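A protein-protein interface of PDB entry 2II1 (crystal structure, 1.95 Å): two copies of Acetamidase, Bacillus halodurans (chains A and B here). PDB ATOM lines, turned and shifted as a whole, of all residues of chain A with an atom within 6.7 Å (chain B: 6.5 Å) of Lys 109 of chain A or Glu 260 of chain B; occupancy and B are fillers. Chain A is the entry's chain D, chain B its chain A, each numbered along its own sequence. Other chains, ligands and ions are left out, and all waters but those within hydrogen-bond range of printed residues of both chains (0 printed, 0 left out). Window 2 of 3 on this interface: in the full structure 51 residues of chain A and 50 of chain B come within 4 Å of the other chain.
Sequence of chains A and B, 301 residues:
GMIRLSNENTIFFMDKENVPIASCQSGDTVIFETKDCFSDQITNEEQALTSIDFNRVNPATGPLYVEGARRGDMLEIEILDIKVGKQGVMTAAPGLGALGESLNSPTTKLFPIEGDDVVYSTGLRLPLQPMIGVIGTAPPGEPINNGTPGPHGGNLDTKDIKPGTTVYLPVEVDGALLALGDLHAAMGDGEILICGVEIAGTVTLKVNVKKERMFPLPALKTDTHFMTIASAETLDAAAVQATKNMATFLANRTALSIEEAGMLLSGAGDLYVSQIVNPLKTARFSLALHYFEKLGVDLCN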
ATOM      1  N   ILE A  42      33.867   6.517  -5.695  1.00  0.00           N
ATOM      2  CA  ILE A  42      33.622   6.024  -7.049  1.00  0.00           C
ATOM      3  C   ILE A  42      33.742   7.187  -8.012  1.00  0.00           C
ATOM      4  O   ILE A  42      32.923   8.102  -7.977  1.00  0.00           O
ATOM      5  CB  ILE A  42      32.243   5.340  -7.214  1.00  0.00           C
ATOM      6  CG1 ILE A  42      32.088   4.189  -6.209  1.00  0.00           C
ATOM      7  CG2 ILE A  42      32.079   4.847  -8.671  1.00  0.00           C
ATOM      8  CD1 ILE A  42      30.770   3.453  -6.299  1.00  0.00           C
ATOM      9  N   ASN A  44      34.940   6.544 -11.547  1.00  0.00           N
ATOM     10  CA  ASN A  44      34.912   6.077 -12.938  1.00  0.00           C
ATOM     11  C   ASN A  44      33.961   4.884 -13.082  1.00  0.00           C
ATOM     12  O   ASN A  44      33.618   4.230 -12.084  1.00  0.00           O
ATOM     13  CB  ASN A  44      36.334   5.761 -13.441  1.00  0.00           C
ATOM     14  CG  ASN A  44      36.845   4.424 -12.960  1.00  0.00           C
ATOM     15  OD1 ASN A  44      36.516   3.384 -13.531  1.00  0.00           O
ATOM     16  ND2 ASN A  44      37.650   4.438 -11.909  1.00  0.00           N
ATOM     17  N   GLU A  45      33.534   4.627 -14.322  1.00  0.00           N
ATOM     18  CA  GLU A  45      32.482   3.644 -14.633  1.00  0.00           C
ATOM     19  C   GLU A  45      32.984   2.186 -14.716  1.00  0.00           C
ATOM     20  O   GLU A  45      32.182   1.254 -14.808  1.00  0.00           O
ATOM     21  CB  GLU A  45      31.776   4.021 -15.940  1.00  0.00           C
ATOM     22  CG  GLU A  45      31.175   5.402 -15.923  1.00  0.00           C
ATOM     23  CD  GLU A  45      30.440   5.760 -17.205  1.00  0.00           C
ATOM     24  OE1 GLU A  45      31.071   5.706 -18.298  1.00  0.00           O
ATOM     25  OE2 GLU A  45      29.230   6.111 -17.112  1.00  0.00           O
ATOM     26  N   GLY A  88      26.970  12.885 -10.936  1.00  0.00           N
ATOM     27  CA  GLY A  88      26.520  11.867 -10.004  1.00  0.00           C
ATOM     28  C   GLY A  88      26.790  10.437 -10.420  1.00  0.00           C
ATOM     29  O   GLY A  88      27.241  10.177 -11.521  1.00  0.00           O
ATOM     30  N   VAL A  89      26.485   9.504  -9.525  1.00  0.00           N
ATOM     31  CA  VAL A  89      26.797   8.079  -9.724  1.00  0.00           C
ATOM     32  C   VAL A  89      25.642   7.168  -9.325  1.00  0.00           C
ATOM     33  O   VAL A  89      24.925   7.463  -8.374  1.00  0.00           O
ATOM     34  CB  VAL A  89      27.997   7.675  -8.852  1.00  0.00           C
ATOM     35  CG1 VAL A  89      28.196   6.128  -8.830  1.00  0.00           C
ATOM     36  CG2 VAL A  89      29.258   8.386  -9.310  1.00  0.00           C
ATOM     37  N   MET A  90      25.442   6.091 -10.078  1.00  0.00           N
ATOM     38  CA  MET A  90      24.570   4.981  -9.661  1.00  0.00           C
ATOM     39  C   MET A  90      25.291   3.648  -9.794  1.00  0.00           C
ATOM     40  O   MET A  90      26.189   3.473 -10.634  1.00  0.00           O
ATOM     41  CB  MET A  90      23.274   4.904 -10.472  1.00  0.00           C
ATOM     42  CG  MET A  90      22.438   6.174 -10.485  1.00  0.00           C
ATOM     43  SD  MET A  90      20.629   5.833 -11.283  1.00  0.00           S
ATOM     44  CE  MET A  90      19.502   6.082  -9.732  1.00  0.00           C
ATOM     45  N   THR A  91      24.878   2.702  -8.954  1.00  0.00           N
ATOM     46  CA  THR A  91      25.452   1.374  -8.949  1.00  0.00           C
ATOM     47  C   THR A  91      24.301   0.381  -8.961  1.00  0.00           C
ATOM     48  O   THR A  91      23.326   0.534  -8.220  1.00  0.00           O
ATOM     49  CB  THR A  91      26.332   1.138  -7.721  1.00  0.00           C
ATOM     50  OG1 THR A  91      25.557   1.328  -6.527  1.00  0.00           O
ATOM     51  CG2 THR A  91      27.489   2.089  -7.718  1.00  0.00           C
ATOM     52  N   ALA A  92      24.387  -0.588  -9.853  1.00  0.00           N
ATOM     53  CA  ALA A  92      23.477  -1.730  -9.855  1.00  0.00           C
ATOM     54  C   ALA A  92      24.301  -2.926  -9.383  1.00  0.00           C
ATOM     55  O   ALA A  92      25.403  -3.153  -9.882  1.00  0.00           O
ATOM     56  CB  ALA A  92      22.881  -1.961 -11.278  1.00  0.00           C
ATOM     57  N   LEU A 103      18.721  -8.623 -11.606  1.00  0.00           N
ATOM     58  CA  LEU A 103      19.951  -8.050 -12.208  1.00  0.00           C
ATOM     59  C   LEU A 103      20.972  -9.160 -12.499  1.00  0.00           C
ATOM     60  O   LEU A 103      21.021 -10.183 -11.785  1.00  0.00           O
ATOM     61  CB  LEU A 103      20.550  -6.954 -11.301  1.00  0.00           C
ATOM     62  CG  LEU A 103      19.578  -5.825 -10.956  1.00  0.00           C
ATOM     63  CD1 LEU A 103      20.090  -5.026  -9.780  1.00  0.00           C
ATOM     64  CD2 LEU A 103      19.359  -4.922 -12.189  1.00  0.00           C
ATOM     65  N   THR A 107      26.898  -2.881 -12.339  1.00  0.00           N
ATOM     66  CA  THR A 107      27.056  -1.758 -13.264  1.00  0.00           C
ATOM     67  C   THR A 107      27.246  -0.458 -12.491  1.00  0.00           C
ATOM     68  O   THR A 107      26.521  -0.203 -11.542  1.00  0.00           O
ATOM     69  CB  THR A 107      25.821  -1.614 -14.192  1.00  0.00           C
ATOM     70  OG1 THR A 107      25.598  -2.851 -14.880  1.00  0.00           O
ATOM     71  CG2 THR A 107      26.045  -0.532 -15.213  1.00  0.00           C
ATOM     72  N   THR A 108      28.253   0.321 -12.878  1.00  0.00           N
ATOM     73  CA  THR A 108      28.462   1.676 -12.382  1.00  0.00           C
ATOM     74  C   THR A 108      28.207   2.634 -13.570  1.00  0.00           C
ATOM     75  O   THR A 108      28.661   2.379 -14.689  1.00  0.00           O
ATOM     76  CB  THR A 108      29.870   1.847 -11.815  1.00  0.00           C
ATOM     77  OG1 THR A 108      30.057   0.973 -10.690  1.00  0.00           O
ATOM     78  CG2 THR A 108      30.100   3.271 -11.371  1.00  0.00           C
ATOM     79  N   LYS A 109      27.446   3.701 -13.326  1.00  0.00           N
ATOM     80  CA  LYS A 109      27.136   4.710 -14.341  1.00  0.00           C
ATOM     81  C   LYS A 109      27.392   6.082 -13.722  1.00  0.00           C
ATOM     82  O   LYS A 109      26.939   6.362 -12.605  1.00  0.00           O
ATOM     83  CB  LYS A 109      25.673   4.585 -14.833  1.00  0.00           C
ATOM     84  CG  LYS A 109      25.328   5.385 -16.119  1.00  0.00           C
ATOM     85  CD  LYS A 109      23.880   5.116 -16.649  1.00  0.00           C
ATOM     86  CE  LYS A 109      23.745   5.150 -18.201  1.00  0.00           C
ATOM     87  NZ  LYS A 109      23.723   3.793 -18.955  1.00  0.00           N
ATOM     88  N   LEU A 110      28.132   6.930 -14.443  1.00  0.00           N
ATOM     89  CA  LEU A 110      28.316   8.336 -14.059  1.00  0.00           C
ATOM     90  C   LEU A 110      27.303   9.214 -14.826  1.00  0.00           C
ATOM     91  O   LEU A 110      27.023   8.976 -16.006  1.00  0.00           O
ATOM     92  CB  LEU A 110      29.758   8.810 -14.328  1.00  0.00           C
ATOM     93  CG  LEU A 110      30.896   8.141 -13.538  1.00  0.00           C
ATOM     94  CD1 LEU A 110      32.274   8.586 -14.041  1.00  0.00           C
ATOM     95  CD2 LEU A 110      30.746   8.454 -12.085  1.00  0.00           C
ATOM     96  N   PHE A 111      26.779  10.230 -14.153  1.00  0.00           N
ATOM     97  CA  PHE A 111      25.744  11.101 -14.713  1.00  0.00           C
ATOM     98  C   PHE A 111      26.222  12.565 -14.684  1.00  0.00           C
ATOM     99  O   PHE A 111      26.159  13.199 -13.632  1.00  0.00           O
ATOM    100  CB  PHE A 111      24.456  10.978 -13.863  1.00  0.00           C
ATOM    101  CG  PHE A 111      23.807   9.614 -13.917  1.00  0.00           C
ATOM    102  CD1 PHE A 111      24.340   8.522 -13.220  1.00  0.00           C
ATOM    103  CD2 PHE A 111      22.657   9.418 -14.668  1.00  0.00           C
ATOM    104  CE1 PHE A 111      23.747   7.282 -13.299  1.00  0.00           C
ATOM    105  CE2 PHE A 111      22.059   8.170 -14.748  1.00  0.00           C
ATOM    106  CZ  PHE A 111      22.595   7.101 -14.051  1.00  0.00           C
ATOM    107  N   VAL A 119      22.140  13.790 -16.912  1.00  0.00           N
ATOM    108  CA  VAL A 119      22.297  13.116 -18.173  1.00  0.00           C
ATOM    109  C   VAL A 119      22.461  11.614 -17.941  1.00  0.00           C
ATOM    110  O   VAL A 119      23.492  11.173 -17.452  1.00  0.00           O
ATOM    111  CB  VAL A 119      23.463  13.686 -19.014  1.00  0.00           C
ATOM    112  CG1 VAL A 119      23.479  13.033 -20.360  1.00  0.00           C
ATOM    113  CG2 VAL A 119      23.328  15.214 -19.179  1.00  0.00           C
ATOM    114  N   TYR A 120      21.419  10.866 -18.311  1.00  0.00           N
ATOM    115  CA  TYR A 120      21.400   9.413 -18.279  1.00  0.00           C
ATOM    116  C   TYR A 120      22.092   8.830 -19.525  1.00  0.00           C
ATOM    117  O   TYR A 120      22.899   7.916 -19.429  1.00  0.00           O
ATOM    118  CB  TYR A 120      19.924   8.935 -18.153  1.00  0.00           C
ATOM    119  CG  TYR A 120      19.763   7.433 -18.176  1.00  0.00           C
ATOM    120  CD1 TYR A 120      19.675   6.753 -19.381  1.00  0.00           C
ATOM    121  CD2 TYR A 120      19.722   6.684 -16.994  1.00  0.00           C
ATOM    122  CE1 TYR A 120      19.564   5.374 -19.429  1.00  0.00           C
ATOM    123  CE2 TYR A 120      19.617   5.306 -17.030  1.00  0.00           C
ATOM    124  CZ  TYR A 120      19.533   4.658 -18.260  1.00  0.00           C
ATOM    125  OH  TYR A 120      19.401   3.302 -18.353  1.00  0.00           O
ATOM    126  N   SER A 121      21.755   9.359 -20.701  1.00  0.00           N
ATOM    127  CA  SER A 121      22.433   9.011 -21.930  1.00  0.00           C
ATOM    128  C   SER A 121      22.155  10.122 -22.927  1.00  0.00           C
ATOM    129  O   SER A 121      21.454  11.074 -22.605  1.00  0.00           O
ATOM    130  CB  SER A 121      21.947   7.666 -22.465  1.00  0.00           C
ATOM    131  OG  SER A 121      20.567   7.689 -22.784  1.00  0.00           O
ATOM    132  N   VAL A 197      20.550   9.061  -7.983  1.00  0.00           N
ATOM    133  CA  VAL A 197      21.766   9.588  -8.598  1.00  0.00           C
ATOM    134  C   VAL A 197      22.529  10.285  -7.485  1.00  0.00           C
ATOM    135  O   VAL A 197      22.201  11.412  -7.103  1.00  0.00           O
ATOM    136  CB  VAL A 197      21.513  10.531  -9.785  1.00  0.00           C
ATOM    137  CG1 VAL A 197      22.863  11.001 -10.342  1.00  0.00           C
ATOM    138  CG2 VAL A 197      20.675   9.815 -10.857  1.00  0.00           C
ATOM    139  N   ALA B 255      15.922  -1.244 -26.055  1.00  0.00           N
ATOM    140  CA  ALA B 255      17.372  -1.426 -26.097  1.00  0.00           C
ATOM    141  C   ALA B 255      18.011  -1.408 -24.720  1.00  0.00           C
ATOM    142  O   ALA B 255      19.159  -1.817 -24.594  1.00  0.00           O
ATOM    143  CB  ALA B 255      18.015  -0.369 -26.969  1.00  0.00           C
ATOM    144  N   LEU B 256      17.301  -0.928 -23.691  1.00  0.00           N
ATOM    145  CA  LEU B 256      17.837  -0.950 -22.316  1.00  0.00           C
ATOM    146  C   LEU B 256      18.120  -2.390 -21.870  1.00  0.00           C
ATOM    147  O   LEU B 256      17.382  -3.299 -22.237  1.00  0.00           O
ATOM    148  CB  LEU B 256      16.857  -0.308 -21.297  1.00  0.00           C
ATOM    149  CG  LEU B 256      16.470   1.163 -21.459  1.00  0.00           C
ATOM    150  CD1 LEU B 256      15.533   1.605 -20.340  1.00  0.00           C
ATOM    151  CD2 LEU B 256      17.673   2.069 -21.497  1.00  0.00           C
ATOM    152  N   SER B 257      19.177  -2.589 -21.082  1.00  0.00           N
ATOM    153  CA  SER B 257      19.380  -3.852 -20.352  1.00  0.00           C
ATOM    154  C   SER B 257      18.633  -3.718 -19.039  1.00  0.00           C
ATOM    155  O   SER B 257      18.103  -2.639 -18.728  1.00  0.00           O
ATOM    156  CB  SER B 257      20.859  -4.111 -20.086  1.00  0.00           C
ATOM    157  OG  SER B 257      21.319  -3.186 -19.126  1.00  0.00           O
ATOM    158  N   ILE B 258      18.587  -4.799 -18.258  1.00  0.00           N
ATOM    159  CA  ILE B 258      17.838  -4.792 -16.990  1.00  0.00           C
ATOM    160  C   ILE B 258      18.460  -3.866 -15.921  1.00  0.00           C
ATOM    161  O   ILE B 258      17.757  -3.293 -15.066  1.00  0.00           O
ATOM    162  CB  ILE B 258      17.680  -6.239 -16.420  1.00  0.00           C
ATOM    163  CG1 ILE B 258      16.714  -6.264 -15.219  1.00  0.00           C
ATOM    164  CG2 ILE B 258      19.052  -6.885 -16.142  1.00  0.00           C
ATOM    165  CD1 ILE B 258      15.263  -5.926 -15.579  1.00  0.00           C
ATOM    166  N   GLU B 259      19.778  -3.764 -15.950  1.00  0.00           N
ATOM    167  CA  GLU B 259      20.536  -2.835 -15.089  1.00  0.00           C
ATOM    168  C   GLU B 259      20.182  -1.414 -15.449  1.00  0.00           C
ATOM    169  O   GLU B 259      19.867  -0.620 -14.574  1.00  0.00           O
ATOM    170  CB  GLU B 259      22.041  -3.023 -15.285  1.00  0.00           C
ATOM    171  CG  GLU B 259      22.578  -4.398 -14.810  1.00  0.00           C
ATOM    172  CD  GLU B 259      22.310  -5.550 -15.808  1.00  0.00           C
ATOM    173  OE1 GLU B 259      22.020  -5.293 -16.991  1.00  0.00           O
ATOM    174  OE2 GLU B 259      22.369  -6.722 -15.402  1.00  0.00           O
ATOM    175  N   GLU B 260      20.269  -1.085 -16.739  1.00  0.00           N
ATOM    176  CA  GLU B 260      19.897   0.252 -17.234  1.00  0.00           C
ATOM    177  C   GLU B 260      18.436   0.634 -16.960  1.00  0.00           C
ATOM    178  O   GLU B 260      18.132   1.795 -16.621  1.00  0.00           O
ATOM    179  CB  GLU B 260      20.170   0.354 -18.730  1.00  0.00           C
ATOM    180  CG  GLU B 260      21.656   0.438 -19.105  1.00  0.00           C
ATOM    181  CD  GLU B 260      21.864   0.520 -20.615  1.00  0.00           C
ATOM    182  OE1 GLU B 260      21.014   0.003 -21.374  1.00  0.00           O
ATOM    183  OE2 GLU B 260      22.854   1.149 -21.045  1.00  0.00           O
ATOM    184  N   ALA B 261      17.538  -0.324 -17.140  1.00  0.00           N
ATOM    185  CA  ALA B 261      16.124  -0.129 -16.826  1.00  0.00           C
ATOM    186  C   ALA B 261      15.917   0.157 -15.357  1.00  0.00           C
ATOM    187  O   ALA B 261      15.185   1.061 -15.019  1.00  0.00           O
ATOM    188  CB  ALA B 261      15.288  -1.330 -17.270  1.00  0.00           C
ATOM    189  N   GLY B 262      16.585  -0.595 -14.479  1.00  0.00           N
ATOM    190  CA  GLY B 262      16.507  -0.375 -13.045  1.00  0.00           C
ATOM    191  C   GLY B 262      17.019   0.988 -12.595  1.00  0.00           C
ATOM    192  O   GLY B 262      16.472   1.575 -11.659  1.00  0.00           O
ATOM    193  N   MET B 263      18.066   1.485 -13.259  1.00  0.00           N
ATOM    194  CA  MET B 263      18.592   2.828 -13.000  1.00  0.00           C
ATOM    195  C   MET B 263      17.599   3.894 -13.435  1.00  0.00           C
ATOM    196  O   MET B 263      17.384   4.892 -12.738  1.00  0.00           O
ATOM    197  CB  MET B 263      19.918   3.033 -13.718  1.00  0.00           C
ATOM    198  CG  MET B 263      21.047   2.333 -13.068  1.00  0.00           C
ATOM    199  SD  MET B 263      22.675   2.619 -14.044  1.00  0.00           S
ATOM    200  CE  MET B 263      23.883   1.492 -12.884  1.00  0.00           C
ATOM    201  N   LEU B 264      16.974   3.675 -14.578  1.00  0.00           N
ATOM    202  CA  LEU B 264      15.998   4.639 -15.050  1.00  0.00           C
ATOM    203  C   LEU B 264      14.826   4.729 -14.072  1.00  0.00           C
ATOM    204  O   LEU B 264      14.391   5.835 -13.767  1.00  0.00           O
ATOM    205  CB  LEU B 264      15.522   4.333 -16.475  1.00  0.00           C
ATOM    206  CG  LEU B 264      14.523   5.355 -17.014  1.00  0.00           C
ATOM    207  CD1 LEU B 264      15.170   6.715 -17.246  1.00  0.00           C
ATOM    208  CD2 LEU B 264      13.829   4.837 -18.296  1.00  0.00           C
ATOM    209  N   LEU B 265      14.340   3.579 -13.593  1.00  0.00           N
ATOM    210  CA  LEU B 265      13.207   3.512 -12.669  1.00  0.00           C
ATOM    211  C   LEU B 265      13.527   4.161 -11.316  1.00  0.00           C
ATOM    212  O   LEU B 265      12.749   4.973 -10.808  1.00  0.00           O
ATOM    213  CB  LEU B 265      12.790   2.047 -12.418  1.00  0.00           C
ATOM    214  CG  LEU B 265      12.233   1.224 -13.601  1.00  0.00           C
ATOM    215  CD1 LEU B 265      11.521  -0.049 -13.117  1.00  0.00           C
ATOM    216  CD2 LEU B 265      11.337   2.055 -14.470  1.00  0.00           C
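The side-chain hydroxyl (OG) of Ser 257 of chain B sits at hydrogen-bond distance from the side-chain carboxylate (OE1) of Glu 259 of chain B (3.1 Å).
N of Ser 257 of chain B sits at hydrogen-bond distance from OE1 of Glu 260 of chain B (3.2 Å).
N of Met 90 of chain A lies within hydrogen-bond range of O of Lys 109 of chain A (2.9 Å).
The backbone carbonyl oxygen (O) of Thr 107 of chain A sits at hydrogen-bond distance from the backbone NH (N) of Ala 92 of chain A (2.7 Å).
Among the printed residues, merely in contact across the chains: Thr 107 of chain A with Glu 259 of chain B, Thr 107 of chain A with Met 263 of chain B, Lys 109 of chain A with Met 263 of chain B, Leu 103 of chain A with Ile 258 of chain B, Ala 92 of chain A with Met 263 of chain B, Leu 103 of chain A with Glu 259 of chain B, Tyr 120 of chain A with Leu 256 of chain B and Tyr 120 of chain A with Leu 264 of chain B.
No position is printed for both chains.
Of the 11 pairs that touch across the chains among the printed residues, none has its exchanged pair printed and touching as well.
Of chain B, only Glu 260 and Met 263 come within 4 Å of Lys 109 of chain A.
Of the printed residues of chain B, Thr 107 of chain A touches Glu 259 (3.4 Å) and Met 263 (3.4 Å).
Printed residues of chain B within 4 Å of Met 90 of chain A: Met 263 (3.7 Å).
The nearest printed residue of chain B that does not touch Lys 109 of chain A is Leu 256 of chain B (6.8 Å).
The nearest residue of chain A that does not touch Glu 260 of chain B is Thr 107 of chain A (5.9 Å).
The nearest printed residue of chain A that does not touch Ile 258 of chain B is Ala 92 of chain A (6.5 Å).
Hydrophobic or aromatic side chains of chain B that line the printed part of chain A: Leu 256 and Met 263.
Of the 18 printed residues of chain A, 6 touch a printed residue of chain B.
Printed residues of chain A that touch a printed residue of chain B: Met 90, Ala 92, Leu 103, Thr 107, Lys 109 and Tyr 120.
Among the printed residues, 11 pairs touch across the chains.
Among the printed residues, Asp or Glu carboxylates within 4 Å of a Lys or Arg side-chain nitrogen of the other chain: Lys 109 of chain A with Glu 260 of chain B (3.5 Å).
The side-chain carboxylate (OE2) of Glu 260 of chain B lies within salt-bridge range of the side-chain amino group (NZ) of Lys 109 of chain A.
The backbone carbonyl oxygen of Glu 260 of chain B lies within hydrogen-bond range of the side-chain hydroxyl of Tyr 120 of chain A.
SD of Met 90 of chain A lies close to O of Met 263 of chain B, at 3.7 Å.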
